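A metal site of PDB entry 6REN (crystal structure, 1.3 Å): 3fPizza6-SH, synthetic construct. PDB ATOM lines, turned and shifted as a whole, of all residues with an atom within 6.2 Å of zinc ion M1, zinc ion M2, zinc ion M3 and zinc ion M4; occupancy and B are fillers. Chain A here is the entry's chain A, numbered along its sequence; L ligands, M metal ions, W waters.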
ATOM      1  N   SER A  20      -5.097  23.723 -25.643  1.00  0.00           N
ATOM      2  CA  SER A  20      -4.179  22.611 -25.814  1.00  0.00           C
ATOM      3  C   SER A  20      -4.678  21.358 -25.113  1.00  0.00           C
ATOM      4  O   SER A  20      -5.256  20.485 -25.749  1.00  0.00           O
ATOM      5  CB  SER A  20      -2.756  23.005 -25.372  1.00  0.00           C
ATOM      6  OG  SER A  20      -2.701  23.376 -23.994  1.00  0.00           O
ATOM      7  N   GLY A  21      -4.506  21.262 -23.822  1.00  0.00           N
ATOM      8  CA  GLY A  21      -4.988  20.095 -23.124  1.00  0.00           C
ATOM      9  C   GLY A  21      -6.504  20.092 -22.943  1.00  0.00           C
ATOM     10  O   GLY A  21      -7.146  21.142 -22.802  1.00  0.00           O
ATOM     11  N   HIS A  35      -3.903  27.669 -23.288  1.00  0.00           N
ATOM     12  CA  HIS A  35      -2.433  27.733 -23.191  1.00  0.00           C
ATOM     13  C   HIS A  35      -1.916  29.155 -23.308  1.00  0.00           C
ATOM     14  O   HIS A  35      -1.028  29.561 -22.535  1.00  0.00           O
ATOM     15  CB  HIS A  35      -1.897  26.858 -24.328  1.00  0.00           C
ATOM     16  CG  HIS A  35      -0.446  26.489 -24.335  1.00  0.00           C
ATOM     17  ND1 HIS A  35       0.542  27.255 -24.935  1.00  0.00           N
ATOM     18  CD2 HIS A  35       0.154  25.313 -24.014  1.00  0.00           C
ATOM     19  CE1 HIS A  35       1.693  26.605 -24.887  1.00  0.00           C
ATOM     20  NE2 HIS A  35       1.489  25.407 -24.340  1.00  0.00           N
ATOM     21  N   THR A  60       2.123  29.095 -19.808  1.00  0.00           N
ATOM     22  CA  THR A  60       1.890  28.053 -20.801  1.00  0.00           C
ATOM     23  C   THR A  60       1.468  26.716 -20.175  1.00  0.00           C
ATOM     24  O   THR A  60       2.135  25.690 -20.337  1.00  0.00           O
ATOM     25  CB  THR A  60       3.012  27.855 -21.813  1.00  0.00           C
ATOM     26  OG1 THR A  60       4.271  27.638 -21.180  1.00  0.00           O
ATOM     27  CG2 THR A  60       3.126  29.122 -22.683  1.00  0.00           C
ATOM     28  N   PRO A  61       0.358  26.699 -19.438  1.00  0.00           N
ATOM     29  CA  PRO A  61      -0.198  25.415 -18.967  1.00  0.00           C
ATOM     30  C   PRO A  61      -0.599  24.563 -20.152  1.00  0.00           C
ATOM     31  O   PRO A  61      -1.058  25.056 -21.181  1.00  0.00           O
ATOM     32  CB  PRO A  61      -1.421  25.840 -18.143  1.00  0.00           C
ATOM     33  CG  PRO A  61      -1.853  27.132 -18.801  1.00  0.00           C
ATOM     34  CD  PRO A  61      -0.583  27.829 -19.231  1.00  0.00           C
ATOM     35  N   HIS A  62      -0.461  23.248 -20.004  1.00  0.00           N
ATOM     36  CA  HIS A  62      -0.553  22.387 -21.184  1.00  0.00           C
ATOM     37  C   HIS A  62      -1.444  21.175 -20.881  1.00  0.00           C
ATOM     38  O   HIS A  62      -2.631  21.189 -21.153  1.00  0.00           O
ATOM     39  CB  HIS A  62       0.858  22.067 -21.661  1.00  0.00           C
ATOM     40  CG  HIS A  62       0.903  21.448 -23.028  1.00  0.00           C
ATOM     41  ND1 HIS A  62       1.578  22.032 -24.082  1.00  0.00           N
ATOM     42  CD2 HIS A  62       0.339  20.312 -23.492  1.00  0.00           C
ATOM     43  CE1 HIS A  62       1.440  21.248 -25.159  1.00  0.00           C
ATOM     44  NE2 HIS A  62       0.678  20.212 -24.817  1.00  0.00           N
ATOM     45  N   GLY A  63      -0.952  20.137 -20.245  1.00  0.00           N
ATOM     46  CA  GLY A  63      -1.815  18.996 -19.974  1.00  0.00           C
ATOM     47  C   GLY A  63      -2.753  19.274 -18.805  1.00  0.00           C
ATOM     48  O   GLY A  63      -2.437  20.055 -17.885  1.00  0.00           O
ATOM     49  N   HIS A  77       4.138  24.158 -17.764  1.00  0.00           N
ATOM     50  CA  HIS A  77       5.499  23.855 -18.238  1.00  0.00           C
ATOM     51  C   HIS A  77       6.444  25.033 -18.217  1.00  0.00           C
ATOM     52  O   HIS A  77       7.639  24.812 -18.045  1.00  0.00           O
ATOM     53  CB  HIS A  77       5.649  23.004 -19.500  1.00  0.00           C
ATOM     54  CG  HIS A  77       5.088  23.586 -20.758  1.00  0.00           C
ATOM     55  ND1 HIS A  77       5.609  24.707 -21.384  1.00  0.00           N
ATOM     56  CD2 HIS A  77       4.096  23.144 -21.558  1.00  0.00           C
ATOM     57  CE1 HIS A  77       4.950  24.920 -22.509  1.00  0.00           C
ATOM     58  NE2 HIS A  77       4.031  23.983 -22.648  1.00  0.00           N
ATOM     59  N   SER A 104       4.656  18.152 -20.138  1.00  0.00           N
ATOM     60  CA  SER A 104       3.574  18.412 -21.090  1.00  0.00           C
ATOM     61  C   SER A 104       2.274  17.750 -20.729  1.00  0.00           C
ATOM     62  O   SER A 104       1.223  18.339 -20.965  1.00  0.00           O
ATOM     63  CB  SER A 104       4.028  18.060 -22.520  1.00  0.00           C
ATOM     64  OG  SER A 104       4.542  16.747 -22.515  1.00  0.00           O
ATOM     65  N   HIS A 119       8.616  15.919 -20.746  1.00  0.00           N
ATOM     66  CA  HIS A 119       8.886  15.995 -22.184  1.00  0.00           C
ATOM     67  C   HIS A 119      10.371  16.271 -22.469  1.00  0.00           C
ATOM     68  O   HIS A 119      11.010  15.582 -23.296  1.00  0.00           O
ATOM     69  CB  HIS A 119       7.961  17.133 -22.673  1.00  0.00           C
ATOM     70  CG  HIS A 119       7.845  17.341 -24.155  1.00  0.00           C
ATOM     71  ND1 HIS A 119       8.752  18.057 -24.897  1.00  0.00           N
ATOM     72  CD2 HIS A 119       6.778  17.115 -24.960  1.00  0.00           C
ATOM     73  CE1 HIS A 119       8.280  18.212 -26.128  1.00  0.00           C
ATOM     74  NE2 HIS A 119       7.089  17.633 -26.202  1.00  0.00           N
ATOM     75  N   THR A 144      11.177  12.935 -26.300  1.00  0.00           N
ATOM     76  CA  THR A 144      10.121  13.926 -26.103  1.00  0.00           C
ATOM     77  C   THR A 144       8.726  13.300 -25.982  1.00  0.00           C
ATOM     78  O   THR A 144       7.836  13.580 -26.795  1.00  0.00           O
ATOM     79  CB  THR A 144      10.132  15.081 -27.111  1.00  0.00           C
ATOM     80  OG1 THR A 144       9.833  14.588 -28.411  1.00  0.00           O
ATOM     81  CG2 THR A 144      11.451  15.804 -27.138  1.00  0.00           C
ATOM     82  N   PRO A 145       8.520  12.455 -24.983  1.00  0.00           N
ATOM     83  CA  PRO A 145       7.162  11.947 -24.713  1.00  0.00           C
ATOM     84  C   PRO A 145       6.240  13.113 -24.323  1.00  0.00           C
ATOM     85  O   PRO A 145       6.622  13.989 -23.543  1.00  0.00           O
ATOM     86  CB  PRO A 145       7.380  10.983 -23.537  1.00  0.00           C
ATOM     87  CG  PRO A 145       8.593  11.596 -22.790  1.00  0.00           C
ATOM     88  CD  PRO A 145       9.484  12.128 -23.906  1.00  0.00           C
ATOM     89  N   HIS A 146       5.033  13.105 -24.875  1.00  0.00           N
ATOM     90  CA  HIS A 146       4.206  14.311 -24.902  1.00  0.00           C
ATOM     91  C   HIS A 146       2.879  14.107 -24.184  1.00  0.00           C
ATOM     92  O   HIS A 146       2.660  14.723 -23.121  1.00  0.00           O
ATOM     93  CB  HIS A 146       4.050  14.758 -26.365  1.00  0.00           C
ATOM     94  CG  HIS A 146       3.283  16.045 -26.534  1.00  0.00           C
ATOM     95  ND1 HIS A 146       3.854  17.221 -26.968  1.00  0.00           N
ATOM     96  CD2 HIS A 146       1.974  16.328 -26.261  1.00  0.00           C
ATOM     97  CE1 HIS A 146       2.933  18.163 -26.978  1.00  0.00           C
ATOM     98  NE2 HIS A 146       1.780  17.667 -26.554  1.00  0.00           N
ATOM     99  N   GLY A 147       1.983  13.286 -24.724  1.00  0.00           N
ATOM    100  CA  GLY A 147       0.691  13.012 -24.124  1.00  0.00           C
ATOM    101  C   GLY A 147       0.780  11.753 -23.282  1.00  0.00           C
ATOM    102  O   GLY A 147       1.572  10.853 -23.577  1.00  0.00           O
ATOM    103  N   HIS A 161       6.631  11.226 -29.334  1.00  0.00           N
ATOM    104  CA  HIS A 161       6.637  11.768 -30.695  1.00  0.00           C
ATOM    105  C   HIS A 161       8.030  11.974 -31.266  1.00  0.00           C
ATOM    106  O   HIS A 161       8.141  12.044 -32.487  1.00  0.00           O
ATOM    107  CB  HIS A 161       5.680  12.969 -30.902  1.00  0.00           C
ATOM    108  CG  HIS A 161       6.116  14.266 -30.243  1.00  0.00           C
ATOM    109  ND1 HIS A 161       7.281  14.953 -30.549  1.00  0.00           N
ATOM    110  CD2 HIS A 161       5.452  15.048 -29.362  1.00  0.00           C
ATOM    111  CE1 HIS A 161       7.337  16.071 -29.826  1.00  0.00           C
ATOM    112  NE2 HIS A 161       6.232  16.158 -29.091  1.00  0.00           N
ATOM    113  N   PRO A 187       2.535  12.524 -33.123  1.00  0.00           N
ATOM    114  CA  PRO A 187       1.313  12.518 -32.300  1.00  0.00           C
ATOM    115  C   PRO A 187       1.433  13.374 -31.039  1.00  0.00           C
ATOM    116  O   PRO A 187       2.510  13.473 -30.434  1.00  0.00           O
ATOM    117  CB  PRO A 187       1.136  11.043 -31.946  1.00  0.00           C
ATOM    118  CG  PRO A 187       2.525  10.481 -31.984  1.00  0.00           C
ATOM    119  CD  PRO A 187       3.205  11.204 -33.130  1.00  0.00           C
ATOM    120  N   SER A 188       0.295  13.973 -30.649  1.00  0.00           N
ATOM    121  CA  SER A 188       0.237  14.839 -29.449  1.00  0.00           C
ATOM    122  C   SER A 188      -0.688  14.222 -28.395  1.00  0.00           C
ATOM    123  O   SER A 188      -0.229  13.474 -27.530  1.00  0.00           O
ATOM    124  CB  SER A 188      -0.150  16.281 -29.834  1.00  0.00           C
ATOM    125  OG  SER A 188      -1.324  16.301 -30.671  1.00  0.00           O
ATOM    126  N   GLY A 189      -1.975  14.532 -28.374  1.00  0.00           N
ATOM    127  CA  GLY A 189      -2.840  13.987 -27.335  1.00  0.00           C
ATOM    128  C   GLY A 189      -3.075  12.498 -27.502  1.00  0.00           C
ATOM    129  O   GLY A 189      -3.093  11.949 -28.614  1.00  0.00           O
ATOM    130  N   HIS A 203      -1.043  14.917 -34.951  1.00  0.00           N
ATOM    131  CA  HIS A 203      -0.975  16.370 -35.091  1.00  0.00           C
ATOM    132  C   HIS A 203      -0.473  16.793 -36.458  1.00  0.00           C
ATOM    133  O   HIS A 203      -0.986  17.742 -37.049  1.00  0.00           O
ATOM    134  CB  HIS A 203      -0.062  16.909 -33.974  1.00  0.00           C
ATOM    135  CG  HIS A 203      -0.173  18.383 -33.703  1.00  0.00           C
ATOM    136  ND1 HIS A 203       0.213  19.376 -34.593  1.00  0.00           N
ATOM    137  CD2 HIS A 203      -0.580  19.026 -32.582  1.00  0.00           C
ATOM    138  CE1 HIS A 203       0.034  20.568 -34.020  1.00  0.00           C
ATOM    139  NE2 HIS A 203      -0.408  20.384 -32.784  1.00  0.00           N
ATOM    140  N   THR A 228      -6.152  22.706 -36.710  1.00  0.00           N
ATOM    141  CA  THR A 228      -4.937  22.192 -36.057  1.00  0.00           C
ATOM    142  C   THR A 228      -5.329  21.525 -34.735  1.00  0.00           C
ATOM    143  O   THR A 228      -5.158  22.100 -33.648  1.00  0.00           O
ATOM    144  CB  THR A 228      -3.888  23.304 -35.878  1.00  0.00           C
ATOM    145  OG1 THR A 228      -3.688  23.968 -37.138  1.00  0.00           O
ATOM    146  CG2 THR A 228      -2.546  22.757 -35.422  1.00  0.00           C
ATOM    147  N   PRO A 229      -5.880  20.326 -34.780  1.00  0.00           N
ATOM    148  CA  PRO A 229      -6.241  19.622 -33.534  1.00  0.00           C
ATOM    149  C   PRO A 229      -5.002  19.273 -32.718  1.00  0.00           C
ATOM    150  O   PRO A 229      -3.892  19.088 -33.249  1.00  0.00           O
ATOM    151  CB  PRO A 229      -6.948  18.361 -34.047  1.00  0.00           C
ATOM    152  CG  PRO A 229      -6.355  18.120 -35.430  1.00  0.00           C
ATOM    153  CD  PRO A 229      -6.209  19.528 -35.983  1.00  0.00           C
ATOM    154  N   HIS A 230      -5.188  19.175 -31.387  1.00  0.00           N
ATOM    155  CA  HIS A 230      -4.054  18.988 -30.495  1.00  0.00           C
ATOM    156  C   HIS A 230      -4.349  17.986 -29.390  1.00  0.00           C
ATOM    157  O   HIS A 230      -3.725  16.912 -29.319  1.00  0.00           O
ATOM    158  CB  HIS A 230      -3.547  20.336 -29.946  1.00  0.00           C
ATOM    159  CG  HIS A 230      -2.288  20.181 -29.159  1.00  0.00           C
ATOM    160  ND1 HIS A 230      -1.049  20.586 -29.590  1.00  0.00           N
ATOM    161  CD2 HIS A 230      -2.093  19.590 -27.949  1.00  0.00           C
ATOM    162  CE1 HIS A 230      -0.132  20.210 -28.693  1.00  0.00           C
ATOM    163  NE2 HIS A 230      -0.736  19.592 -27.678  1.00  0.00           N
ATOM    164  N   GLY A 231      -5.253  18.326 -28.481  1.00  0.00           N
ATOM    165  CA  GLY A 231      -5.579  17.447 -27.369  1.00  0.00           C
ATOM    166  C   GLY A 231      -6.814  16.619 -27.664  1.00  0.00           C
ATOM    167  O   GLY A 231      -7.681  17.019 -28.472  1.00  0.00           O
ATOM    168  N   HIS A 245      -6.298  24.398 -31.889  1.00  0.00           N
ATOM    169  CA  HIS A 245      -5.676  25.715 -31.733  1.00  0.00           C
ATOM    170  C   HIS A 245      -5.441  26.421 -33.054  1.00  0.00           C
ATOM    171  O   HIS A 245      -4.925  27.548 -33.053  1.00  0.00           O
ATOM    172  CB  HIS A 245      -4.426  25.705 -30.830  1.00  0.00           C
ATOM    173  CG  HIS A 245      -3.293  24.814 -31.279  1.00  0.00           C
ATOM    174  ND1 HIS A 245      -2.522  25.076 -32.386  1.00  0.00           N
ATOM    175  CD2 HIS A 245      -2.789  23.685 -30.727  1.00  0.00           C
ATOM    176  CE1 HIS A 245      -1.610  24.134 -32.512  1.00  0.00           C
ATOM    177  NE2 HIS A 245      -1.737  23.269 -31.513  1.00  0.00           N
HETATM  178  C1  LIG L   1       1.366  23.172 -32.734  1.00  0.00           C
HETATM  179  C2  LIG L   1       2.198  22.695 -31.606  1.00  0.00           C
HETATM  180  C3  LIG L   1       3.401  23.508 -31.177  1.00  0.00           C
HETATM  181  O1  LIG L   1       1.349  22.171 -30.701  1.00  0.00           O
HETATM  182  C1  LG2 L   2       7.756  19.085 -29.090  1.00  0.00           C
HETATM  183  C2  LG2 L   2       6.580  19.911 -29.038  1.00  0.00           C
HETATM  184  C3  LG2 L   2       6.569  21.209 -29.818  1.00  0.00           C
HETATM  185  O1  LG2 L   2       5.463  19.399 -28.530  1.00  0.00           O
HETATM  186  C1  LG3 L   3       5.133  24.498 -27.649  1.00  0.00           C
HETATM  187  C2  LG3 L   3       4.217  24.821 -26.478  1.00  0.00           C
HETATM  188  C3  LG3 L   3       4.882  25.819 -25.545  1.00  0.00           C
HETATM  189  O1  LG3 L   3       3.695  23.674 -25.835  1.00  0.00           O
HETATM  190 ZN    ZN M   1      -0.500  21.674 -31.237  1.00  0.00          ZN
HETATM  191 ZN    ZN M   2       0.127  18.741 -26.110  1.00  0.00          ZN
HETATM  192 ZN    ZN M   3       5.726  17.581 -27.735  1.00  0.00          ZN
HETATM  193 ZN    ZN M   4       2.689  23.753 -24.150  1.00  0.00          ZN
HETATM  194  O   HOH W   1      -1.567  17.279 -25.411  1.00  0.00           O
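The side-chain hydroxyl of Ser 188 lies within hydrogen-bond range of the backbone carbonyl oxygen of His 230 (2.8 Å).
The backbone carbonyl oxygen (O) of His 230 lies within hydrogen-bond range of the backbone NH (N) of Gly 189 (3.1 Å).
O of His 146 is in hydrogen-bond range of OG of Ser 104 (2.8 Å).
OG1 of Thr 60 sits close to ND1 of His 77.
The side-chain hydroxyl (OG1) of Thr 144 sits close to a ring nitrogen (ND1) of His 161 (3.3 Å).
The backbone NH (N) of Gly 21 lies close to the backbone carbonyl oxygen (O) of His 62 (3.3 Å).
N of His 245 is in hydrogen-bond range of O of Thr 228.
Within 4 Å of zinc ion M1: His 203, His 230 and His 245.
The nearest printed residue that does not touch zinc ion M1 is Pro 229 (4.7 Å).
The nearest printed residue that does not touch zinc ion M2 is Ser 188 (4.5 Å).
Within 4 Å of zinc ion M3: His 119, His 146 and His 161.
Zinc ion M1 is bound by O1 of LIG L1, NE2 of His 203, NE2 of His 245 and ND1 of His 230.
Zinc ion M2 is bound by a ring nitrogen (NE2) of His 230 (2.0 Å), a ring nitrogen (NE2) of His 146 (2.0 Å), a ring nitrogen (NE2) of His 62 (2.0 Å) and water W1 (2.3 Å).
Zinc ion M2 has four donor atoms within binding distance.
O1 of LG2 L2 binds zinc ion M3, at 2.0 Å.
NE2 of His 161 binds zinc ion M3 (2.0 Å).
NE2 of His 119 binds zinc ion M3 (2.1 Å).
Zinc ion M3 is bound by ND1 of His 146.
Zinc ion M4 is bound by O1 of LG3 L3 (2.0 Å).
A ring nitrogen (NE2) of His 77 binds zinc ion M4, at 2.0 Å.
A ring nitrogen (ND1) of His 62 is bound to zinc ion M4, at 2.0 Å.
Zinc ion M4 is bound by NE2 of His 35, 2.1 Å away.
Zinc ion M4 has four donor atoms within binding distance.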
